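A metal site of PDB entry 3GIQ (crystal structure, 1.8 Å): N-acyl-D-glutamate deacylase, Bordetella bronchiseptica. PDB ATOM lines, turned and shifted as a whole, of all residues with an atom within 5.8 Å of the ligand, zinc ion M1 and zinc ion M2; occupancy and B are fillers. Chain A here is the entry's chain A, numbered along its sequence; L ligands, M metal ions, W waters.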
ATOM      1  N   HIS A  66     -23.005   9.360  19.485  1.00  0.00           N
ATOM      2  CA  HIS A  66     -21.796   9.208  20.276  1.00  0.00           C
ATOM      3  C   HIS A  66     -20.643   8.627  19.467  1.00  0.00           C
ATOM      4  O   HIS A  66     -20.296   7.454  19.603  1.00  0.00           O
ATOM      5  CB  HIS A  66     -22.038   8.325  21.504  1.00  0.00           C
ATOM      6  CG  HIS A  66     -20.992   8.498  22.563  1.00  0.00           C
ATOM      7  ND1 HIS A  66     -21.163   9.356  23.635  1.00  0.00           N
ATOM      8  CD2 HIS A  66     -19.736   8.004  22.672  1.00  0.00           C
ATOM      9  CE1 HIS A  66     -20.051   9.371  24.361  1.00  0.00           C
ATOM     10  NE2 HIS A  66     -19.175   8.559  23.791  1.00  0.00           N
ATOM     11  N   GLY A  67     -20.065   9.459  18.618  1.00  0.00           N
ATOM     12  CA  GLY A  67     -18.946   9.008  17.810  1.00  0.00           C
ATOM     13  C   GLY A  67     -17.615   9.562  18.300  1.00  0.00           C
ATOM     14  O   GLY A  67     -17.568  10.579  19.004  1.00  0.00           O
ATOM     15  N   HIS A  68     -16.544   8.859  17.949  1.00  0.00           N
ATOM     16  CA  HIS A  68     -15.184   9.274  18.288  1.00  0.00           C
ATOM     17  C   HIS A  68     -14.384   9.200  16.987  1.00  0.00           C
ATOM     18  O   HIS A  68     -13.176   8.942  16.996  1.00  0.00           O
ATOM     19  CB  HIS A  68     -14.576   8.335  19.341  1.00  0.00           C
ATOM     20  CG  HIS A  68     -15.032   8.614  20.739  1.00  0.00           C
ATOM     21  ND1 HIS A  68     -14.832   9.821  21.367  1.00  0.00           N
ATOM     22  CD2 HIS A  68     -15.711   7.839  21.625  1.00  0.00           C
ATOM     23  CE1 HIS A  68     -15.357   9.778  22.577  1.00  0.00           C
ATOM     24  NE2 HIS A  68     -15.903   8.593  22.758  1.00  0.00           N
ATOM     25  N   ASN A  94     -16.815  13.635  21.532  1.00  0.00           N
ATOM     26  CA  ASN A  94     -17.425  13.228  22.790  1.00  0.00           C
ATOM     27  C   ASN A  94     -16.468  12.929  23.946  1.00  0.00           C
ATOM     28  O   ASN A  94     -15.260  12.808  23.755  1.00  0.00           O
ATOM     29  CB  ASN A  94     -18.307  11.987  22.545  1.00  0.00           C
ATOM     30  CG  ASN A  94     -19.602  12.336  21.841  1.00  0.00           C
ATOM     31  OD1 ASN A  94     -20.513  12.886  22.454  1.00  0.00           O
ATOM     32  ND2 ASN A  94     -19.689  12.036  20.554  1.00  0.00           N
ATOM     33  N   CYS A  95     -17.030  12.816  25.141  1.00  0.00           N
ATOM     34  CA  CYS A  95     -16.283  12.495  26.354  1.00  0.00           C
ATOM     35  C   CYS A  95     -15.088  13.394  26.676  1.00  0.00           C
ATOM     36  O   CYS A  95     -14.094  12.936  27.246  1.00  0.00           O
ATOM     37  CB  CYS A  95     -15.832  11.038  26.283  1.00  0.00           C
ATOM     38  SG  CYS A  95     -17.232   9.920  26.033  1.00  0.00           S
ATOM     39  N   LEU A 114      -7.214   7.870  21.735  1.00  0.00           N
ATOM     40  CA  LEU A 114      -8.289   7.082  21.138  1.00  0.00           C
ATOM     41  C   LEU A 114      -8.814   7.661  19.826  1.00  0.00           C
ATOM     42  O   LEU A 114      -9.415   6.940  19.027  1.00  0.00           O
ATOM     43  CB  LEU A 114      -9.451   6.941  22.123  1.00  0.00           C
ATOM     44  CG  LEU A 114      -9.177   6.144  23.400  1.00  0.00           C
ATOM     45  CD1 LEU A 114     -10.465   6.088  24.236  1.00  0.00           C
ATOM     46  CD2 LEU A 114      -8.714   4.745  23.038  1.00  0.00           C
ATOM     47  N   ALA A 189     -14.568  11.547  34.252  1.00  0.00           N
ATOM     48  CA  ALA A 189     -13.966  10.359  34.846  1.00  0.00           C
ATOM     49  C   ALA A 189     -12.507  10.247  34.412  1.00  0.00           C
ATOM     50  O   ALA A 189     -11.791   9.339  34.830  1.00  0.00           O
ATOM     51  CB  ALA A 189     -14.741   9.110  34.428  1.00  0.00           C
ATOM     52  N   TYR A 190     -12.076  11.179  33.558  1.00  0.00           N
ATOM     53  CA  TYR A 190     -10.714  11.193  33.018  1.00  0.00           C
ATOM     54  C   TYR A 190      -9.950  12.475  33.344  1.00  0.00           C
ATOM     55  O   TYR A 190     -10.542  13.504  33.659  1.00  0.00           O
ATOM     56  CB  TYR A 190     -10.740  11.101  31.487  1.00  0.00           C
ATOM     57  CG  TYR A 190     -11.471   9.922  30.893  1.00  0.00           C
ATOM     58  CD1 TYR A 190     -11.051   8.616  31.129  1.00  0.00           C
ATOM     59  CD2 TYR A 190     -12.550  10.117  30.023  1.00  0.00           C
ATOM     60  CE1 TYR A 190     -11.666   7.532  30.505  1.00  0.00           C
ATOM     61  CE2 TYR A 190     -13.175   9.045  29.391  1.00  0.00           C
ATOM     62  CZ  TYR A 190     -12.722   7.756  29.635  1.00  0.00           C
ATOM     63  OH  TYR A 190     -13.307   6.686  28.996  1.00  0.00           O
ATOM     64  N   HIS A 218     -19.661  12.607  29.941  1.00  0.00           N
ATOM     65  CA  HIS A 218     -19.237  11.290  30.375  1.00  0.00           C
ATOM     66  C   HIS A 218     -19.083  11.712  31.834  1.00  0.00           C
ATOM     67  O   HIS A 218     -18.135  12.421  32.188  1.00  0.00           O
ATOM     68  CB  HIS A 218     -17.879  10.917  29.785  1.00  0.00           C
ATOM     69  CG  HIS A 218     -17.313   9.658  30.365  1.00  0.00           C
ATOM     70  ND1 HIS A 218     -16.634   8.732  29.606  1.00  0.00           N
ATOM     71  CD2 HIS A 218     -17.323   9.179  31.626  1.00  0.00           C
ATOM     72  CE1 HIS A 218     -16.244   7.730  30.379  1.00  0.00           C
ATOM     73  NE2 HIS A 218     -16.647   7.979  31.612  1.00  0.00           N
ATOM     74  N   GLU A 222     -19.162   6.061  36.935  1.00  0.00           N
ATOM     75  CA  GLU A 222     -20.276   5.246  36.483  1.00  0.00           C
ATOM     76  C   GLU A 222     -20.404   3.934  37.252  1.00  0.00           C
ATOM     77  O   GLU A 222     -21.029   2.987  36.791  1.00  0.00           O
ATOM     78  CB  GLU A 222     -20.151   4.977  34.978  1.00  0.00           C
ATOM     79  CG  GLU A 222     -20.122   6.266  34.164  1.00  0.00           C
ATOM     80  CD  GLU A 222     -20.179   6.037  32.674  1.00  0.00           C
ATOM     81  OE1 GLU A 222     -19.228   5.446  32.122  1.00  0.00           O
ATOM     82  OE2 GLU A 222     -21.181   6.437  32.050  1.00  0.00           O
ATOM     83  N   SER A 247     -23.980  10.858  28.388  1.00  0.00           N
ATOM     84  CA  SER A 247     -23.375   9.924  27.453  1.00  0.00           C
ATOM     85  C   SER A 247     -23.281   8.503  27.973  1.00  0.00           C
ATOM     86  O   SER A 247     -23.094   8.278  29.169  1.00  0.00           O
ATOM     87  CB  SER A 247     -21.956  10.396  27.083  1.00  0.00           C
ATOM     88  OG  SER A 247     -21.985  11.691  26.511  1.00  0.00           O
ATOM     89  N   HIS A 248     -23.412   7.547  27.054  1.00  0.00           N
ATOM     90  CA  HIS A 248     -23.346   6.114  27.362  1.00  0.00           C
ATOM     91  C   HIS A 248     -23.725   5.800  28.802  1.00  0.00           C
ATOM     92  O   HIS A 248     -22.929   5.254  29.571  1.00  0.00           O
ATOM     93  CB  HIS A 248     -21.942   5.571  27.052  1.00  0.00           C
ATOM     94  CG  HIS A 248     -20.820   6.378  27.631  1.00  0.00           C
ATOM     95  ND1 HIS A 248     -20.731   6.691  28.979  1.00  0.00           N
ATOM     96  CD2 HIS A 248     -19.709   6.901  27.057  1.00  0.00           C
ATOM     97  CE1 HIS A 248     -19.619   7.367  29.199  1.00  0.00           C
ATOM     98  NE2 HIS A 248     -18.981   7.505  28.054  1.00  0.00           N
ATOM     99  N   LYS A 250     -24.863   4.123  32.042  1.00  0.00           N
ATOM    100  CA  LYS A 250     -24.714   2.739  32.480  1.00  0.00           C
ATOM    101  C   LYS A 250     -24.454   2.678  33.976  1.00  0.00           C
ATOM    102  O   LYS A 250     -24.270   3.706  34.633  1.00  0.00           O
ATOM    103  CB  LYS A 250     -23.491   2.134  31.780  1.00  0.00           C
ATOM    104  CG  LYS A 250     -22.192   2.802  32.248  1.00  0.00           C
ATOM    105  CD  LYS A 250     -20.931   2.148  31.691  1.00  0.00           C
ATOM    106  CE  LYS A 250     -20.696   2.502  30.236  1.00  0.00           C
ATOM    107  NZ  LYS A 250     -20.510   3.977  30.043  1.00  0.00           N
ATOM    108  N   MET A 252     -21.865   0.365  36.263  1.00  0.00           N
ATOM    109  CA  MET A 252     -20.794  -0.621  36.275  1.00  0.00           C
ATOM    110  C   MET A 252     -20.577  -1.287  37.636  1.00  0.00           C
ATOM    111  O   MET A 252     -20.696  -0.638  38.677  1.00  0.00           O
ATOM    112  CB  MET A 252     -19.482   0.019  35.820  1.00  0.00           C
ATOM    113  CG  MET A 252     -19.525   0.528  34.395  1.00  0.00           C
ATOM    114  SD  MET A 252     -17.967   1.291  33.903  1.00  0.00           S
ATOM    115  CE  MET A 252     -16.975  -0.178  33.614  1.00  0.00           C
ATOM    116  N   TYR A 282     -25.110   2.180  24.029  1.00  0.00           N
ATOM    117  CA  TYR A 282     -24.720   1.286  22.952  1.00  0.00           C
ATOM    118  C   TYR A 282     -25.287  -0.015  23.541  1.00  0.00           C
ATOM    119  O   TYR A 282     -25.274  -0.212  24.762  1.00  0.00           O
ATOM    120  CB  TYR A 282     -23.203   1.240  22.754  1.00  0.00           C
ATOM    121  CG  TYR A 282     -22.379   1.188  24.019  1.00  0.00           C
ATOM    122  CD1 TYR A 282     -22.155  -0.016  24.684  1.00  0.00           C
ATOM    123  CD2 TYR A 282     -21.801   2.355  24.530  1.00  0.00           C
ATOM    124  CE1 TYR A 282     -21.373  -0.061  25.837  1.00  0.00           C
ATOM    125  CE2 TYR A 282     -21.015   2.318  25.677  1.00  0.00           C
ATOM    126  CZ  TYR A 282     -20.803   1.101  26.315  1.00  0.00           C
ATOM    127  OH  TYR A 282     -20.019   1.062  27.438  1.00  0.00           O
ATOM    128  N   GLY A 286     -20.557  -4.484  27.938  1.00  0.00           N
ATOM    129  CA  GLY A 286     -19.136  -4.299  28.141  1.00  0.00           C
ATOM    130  C   GLY A 286     -18.761  -2.926  27.630  1.00  0.00           C
ATOM    131  O   GLY A 286     -19.256  -2.499  26.592  1.00  0.00           O
ATOM    132  N   SER A 287     -17.907  -2.209  28.359  1.00  0.00           N
ATOM    133  CA  SER A 287     -17.484  -0.875  27.916  1.00  0.00           C
ATOM    134  C   SER A 287     -16.116  -0.995  27.254  1.00  0.00           C
ATOM    135  O   SER A 287     -15.571  -2.078  27.137  1.00  0.00           O
ATOM    136  CB  SER A 287     -17.413   0.081  29.105  1.00  0.00           C
ATOM    137  OG  SER A 287     -16.388  -0.309  30.012  1.00  0.00           O
ATOM    138  N   SER A 288     -15.580   0.134  26.808  1.00  0.00           N
ATOM    139  CA  SER A 288     -14.258   0.129  26.174  1.00  0.00           C
ATOM    140  C   SER A 288     -13.655   1.521  26.173  1.00  0.00           C
ATOM    141  O   SER A 288     -14.275   2.491  25.739  1.00  0.00           O
ATOM    142  CB  SER A 288     -14.343  -0.404  24.747  1.00  0.00           C
ATOM    143  OG  SER A 288     -13.046  -0.499  24.173  1.00  0.00           O
ATOM    144  N   THR A 289     -12.423   1.615  26.673  1.00  0.00           N
ATOM    145  CA  THR A 289     -11.710   2.881  26.728  1.00  0.00           C
ATOM    146  C   THR A 289     -10.239   2.554  26.983  1.00  0.00           C
ATOM    147  O   THR A 289      -9.798   1.453  26.652  1.00  0.00           O
ATOM    148  CB  THR A 289     -12.268   3.793  27.855  1.00  0.00           C
ATOM    149  OG1 THR A 289     -11.628   5.074  27.806  1.00  0.00           O
ATOM    150  CG2 THR A 289     -12.043   3.167  29.224  1.00  0.00           C
ATOM    151  N   ILE A 292      -7.008   0.812  32.307  1.00  0.00           N
ATOM    152  CA  ILE A 292      -6.844   1.415  33.623  1.00  0.00           C
ATOM    153  C   ILE A 292      -6.366   0.352  34.594  1.00  0.00           C
ATOM    154  O   ILE A 292      -7.139  -0.496  35.038  1.00  0.00           O
ATOM    155  CB  ILE A 292      -8.188   1.997  34.111  1.00  0.00           C
ATOM    156  CG1 ILE A 292      -8.669   3.066  33.127  1.00  0.00           C
ATOM    157  CG2 ILE A 292      -8.039   2.574  35.513  1.00  0.00           C
ATOM    158  CD1 ILE A 292     -10.128   3.488  33.335  1.00  0.00           C
ATOM    159  N   ARG A 295      -8.109  -1.127  37.692  1.00  0.00           N
ATOM    160  CA  ARG A 295      -9.246  -2.035  37.510  1.00  0.00           C
ATOM    161  C   ARG A 295      -8.830  -3.501  37.364  1.00  0.00           C
ATOM    162  O   ARG A 295      -9.675  -4.388  37.351  1.00  0.00           O
ATOM    163  CB  ARG A 295     -10.047  -1.636  36.264  1.00  0.00           C
ATOM    164  CG  ARG A 295     -10.724  -0.289  36.365  1.00  0.00           C
ATOM    165  CD  ARG A 295     -11.516   0.000  35.093  1.00  0.00           C
ATOM    166  NE  ARG A 295     -12.299   1.230  35.197  1.00  0.00           N
ATOM    167  CZ  ARG A 295     -13.123   1.665  34.260  1.00  0.00           C
ATOM    168  NH1 ARG A 295     -13.278   0.979  33.134  1.00  0.00           N
ATOM    169  NH2 ARG A 295     -13.815   2.781  34.445  1.00  0.00           N
ATOM    170  N   TYR A 343     -14.205  -3.751  29.112  1.00  0.00           N
ATOM    171  CA  TYR A 343     -14.561  -4.109  30.481  1.00  0.00           C
ATOM    172  C   TYR A 343     -15.982  -4.653  30.546  1.00  0.00           C
ATOM    173  O   TYR A 343     -16.936  -3.911  30.318  1.00  0.00           O
ATOM    174  CB  TYR A 343     -14.451  -2.860  31.365  1.00  0.00           C
ATOM    175  CG  TYR A 343     -13.099  -2.166  31.309  1.00  0.00           C
ATOM    176  CD1 TYR A 343     -12.042  -2.571  32.116  1.00  0.00           C
ATOM    177  CD2 TYR A 343     -12.897  -1.069  30.456  1.00  0.00           C
ATOM    178  CE1 TYR A 343     -10.808  -1.921  32.089  1.00  0.00           C
ATOM    179  CE2 TYR A 343     -11.656  -0.403  30.418  1.00  0.00           C
ATOM    180  CZ  TYR A 343     -10.620  -0.841  31.238  1.00  0.00           C
ATOM    181  OH  TYR A 343      -9.415  -0.181  31.244  1.00  0.00           O
ATOM    182  N   MET A 346     -21.329  -4.555  33.066  1.00  0.00           N
ATOM    183  CA  MET A 346     -22.713  -4.123  33.144  1.00  0.00           C
ATOM    184  C   MET A 346     -23.698  -5.283  33.050  1.00  0.00           C
ATOM    185  O   MET A 346     -23.342  -6.384  32.643  1.00  0.00           O
ATOM    186  CB  MET A 346     -23.024  -3.099  32.052  1.00  0.00           C
ATOM    187  CG  MET A 346     -22.257  -1.782  32.180  1.00  0.00           C
ATOM    188  SD  MET A 346     -20.727  -1.729  31.230  1.00  0.00           S
ATOM    189  CE  MET A 346     -21.357  -1.286  29.623  1.00  0.00           C
ATOM    190  N   ASP A 365     -20.433   4.618  20.069  1.00  0.00           N
ATOM    191  CA  ASP A 365     -19.214   4.793  20.858  1.00  0.00           C
ATOM    192  C   ASP A 365     -18.088   3.937  20.273  1.00  0.00           C
ATOM    193  O   ASP A 365     -17.235   3.409  20.991  1.00  0.00           O
ATOM    194  CB  ASP A 365     -19.453   4.431  22.318  1.00  0.00           C
ATOM    195  CG  ASP A 365     -18.426   5.066  23.251  1.00  0.00           C
ATOM    196  OD1 ASP A 365     -17.589   5.862  22.772  1.00  0.00           O
ATOM    197  OD2 ASP A 365     -18.453   4.770  24.469  1.00  0.00           O
ATOM    198  N   LEU A 367     -14.652   2.887  18.612  1.00  0.00           N
ATOM    199  CA  LEU A 367     -13.290   3.401  18.735  1.00  0.00           C
ATOM    200  C   LEU A 367     -12.582   2.858  17.493  1.00  0.00           C
ATOM    201  O   LEU A 367     -11.909   1.825  17.536  1.00  0.00           O
ATOM    202  CB  LEU A 367     -12.652   2.880  20.017  1.00  0.00           C
ATOM    203  CG  LEU A 367     -13.414   3.300  21.287  1.00  0.00           C
ATOM    204  CD1 LEU A 367     -12.712   2.770  22.521  1.00  0.00           C
ATOM    205  CD2 LEU A 367     -13.522   4.813  21.343  1.00  0.00           C
ATOM    206  N   ARG A 376     -19.195  -2.877  19.010  1.00  0.00           N
ATOM    207  CA  ARG A 376     -20.171  -1.794  18.878  1.00  0.00           C
ATOM    208  C   ARG A 376     -19.789  -0.865  17.735  1.00  0.00           C
ATOM    209  O   ARG A 376     -20.633  -0.150  17.190  1.00  0.00           O
ATOM    210  CB  ARG A 376     -20.249  -1.000  20.185  1.00  0.00           C
ATOM    211  CG  ARG A 376     -18.991  -0.223  20.521  1.00  0.00           C
ATOM    212  CD  ARG A 376     -19.012   0.238  21.962  1.00  0.00           C
ATOM    213  NE  ARG A 376     -17.873   1.100  22.288  1.00  0.00           N
ATOM    214  CZ  ARG A 376     -17.509   1.419  23.519  1.00  0.00           C
ATOM    215  NH1 ARG A 376     -18.179   0.932  24.559  1.00  0.00           N
ATOM    216  NH2 ARG A 376     -16.481   2.225  23.726  1.00  0.00           N
HETATM  217  C1  LIG L   1     -15.667   2.961  31.486  1.00  0.00           C
HETATM  218  C2  LIG L   1     -16.614   3.521  30.425  1.00  0.00           C
HETATM  219  C3  LIG L   1     -15.846   3.799  29.134  1.00  0.00           C
HETATM  220  C4  LIG L   1     -16.611   4.333  27.883  1.00  0.00           C
HETATM  221  C5  LIG L   1     -17.648   3.275  27.444  1.00  0.00           C
HETATM  222  C6  LIG L   1     -14.067   6.310  25.283  1.00  0.00           C
HETATM  223  P1  LIG L   1     -15.553   6.236  26.269  1.00  0.00           P
HETATM  224  O1  LIG L   1     -16.767   6.599  25.312  1.00  0.00           O
HETATM  225  O2  LIG L   1     -15.447   7.217  27.384  1.00  0.00           O
HETATM  226  N1  LIG L   1     -15.738   4.688  26.721  1.00  0.00           N
HETATM  227  O3  LIG L   1     -17.295   2.375  26.662  1.00  0.00           O
HETATM  228  O4  LIG L   1     -18.792   3.409  27.909  1.00  0.00           O
HETATM  229  O5  LIG L   1     -15.315   1.766  31.361  1.00  0.00           O
HETATM  230  O6  LIG L   1     -15.309   3.749  32.380  1.00  0.00           O
HETATM  231 ZN    ZN M   1     -17.145   8.256  24.263  1.00  0.00          ZN
HETATM  232 ZN    ZN M   2     -17.013   8.379  27.713  1.00  0.00          ZN
HETATM  233  O   HOH W   1     -16.802   5.728  33.243  1.00  0.00           O
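The side-chain carboxylate (OD2) of Asp 365 lies close to an oxygen (O1) of the ligand. The side-chain hydroxyl of Tyr 282 is in hydrogen-bond range of an oxygen (O4) of the ligand, 2.7 Å away. OG of Ser 287 is in hydrogen-bond range of O5 of the ligand. An oxygen (O3) of the ligand lies within salt-bridge range of the guanidinium group (NH1) of Arg 376. The guanidinium group (NH2) of Arg 295 lies within salt-bridge range of an oxygen (O6) of the ligand (2.7 Å). OH of Tyr 190 sits close to O2 of the ligand, 2.7 Å away. An oxygen (O4) of the ligand lies within salt-bridge range of the side-chain amino group (NZ) of Lys 250. N of Ser 288 lies within hydrogen-bond range of O3 of the ligand, at 2.8 Å. N1 of the ligand sits at hydrogen-bond distance from O of Ser 288 (2.8 Å).
Merely in contact with zinc ion M1: Asp 365 (2.9 Å).
Zinc ion M1 is bound by NE2 of His 68 (2.0 Å). O1 of the ligand is bound to zinc ion M1, at 2.0 Å. Zinc ion M1 is bound by NE2 of His 66 (2.1 Å). SG of Cys 95 is bound to zinc ion M1.
SD of Met 252 lies close to O5 of the ligand, at 3.7 Å. CD1 of Leu 114 touches C6 of the ligand, 3.8 Å away. Glu 222 touches the ligand. OG1 of Thr 289 touches C6 of the ligand, at 3.7 Å. CD2 of Tyr 343 touches O5 of the ligand (3.8 Å). Hydrophobic or aromatic side chains that line the ligand: Leu 114, Tyr 190, His 218, His 248, Met 252, Tyr 282 and Tyr 343. Within 4 Å of the ligand: His 66, His 68, Cys 95, Leu 114, Tyr 190, His 218, Glu 222, His 248, Lys 250, Met 252, Tyr 282, Ser 287, Ser 288, Thr 289, Arg 295, Tyr 343, Asp 365 and Arg 376.
Water W1 lies within hydrogen-bond range of O6 of the ligand (2.6 Å), OE1 of Glu 222 (2.7 Å) and NE2 of His 218 (2.8 Å).
Of the 26 residues printed, 3 come within 4 Å of zinc ion M2.
ND1 of His 218 binds zinc ion M2, at 2.0 Å. Zinc ion M2 is bound by O2 of the ligand. Zinc ion M2 is bound by a ring nitrogen (NE2) of His 248 (2.2 Å). Zinc ion M2 is bound by SG of Cys 95. Zinc ion M2 has four donor atoms within binding distance.
OD1 of Asp 365 sits close to NE2 of His 68, at 3.2 Å. The backbone carbonyl oxygen of His 66 is in hydrogen-bond range of the backbone NH of Asp 365 (2.9 Å). The backbone carbonyl oxygen (O) of His 248 lies within hydrogen-bond range of the side-chain amino group (NZ) of Lys 250 (2.8 Å). OE2 of Glu 222 sits at hydrogen-bond distance from ND1 of His 248. OD2 of Asp 365 is in salt-bridge range of NH2 of Arg 376, at 3.3 Å. The side-chain hydroxyl of Tyr 282 sits close to the guanidinium group of Arg 376, at 3.4 Å. OH of Tyr 190 is in hydrogen-bond range of OG1 of Thr 289 (2.6 Å). The backbone NH (N) of Met 252 is in hydrogen-bond range of the backbone carbonyl oxygen (O) of Glu 222 (2.8 Å).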
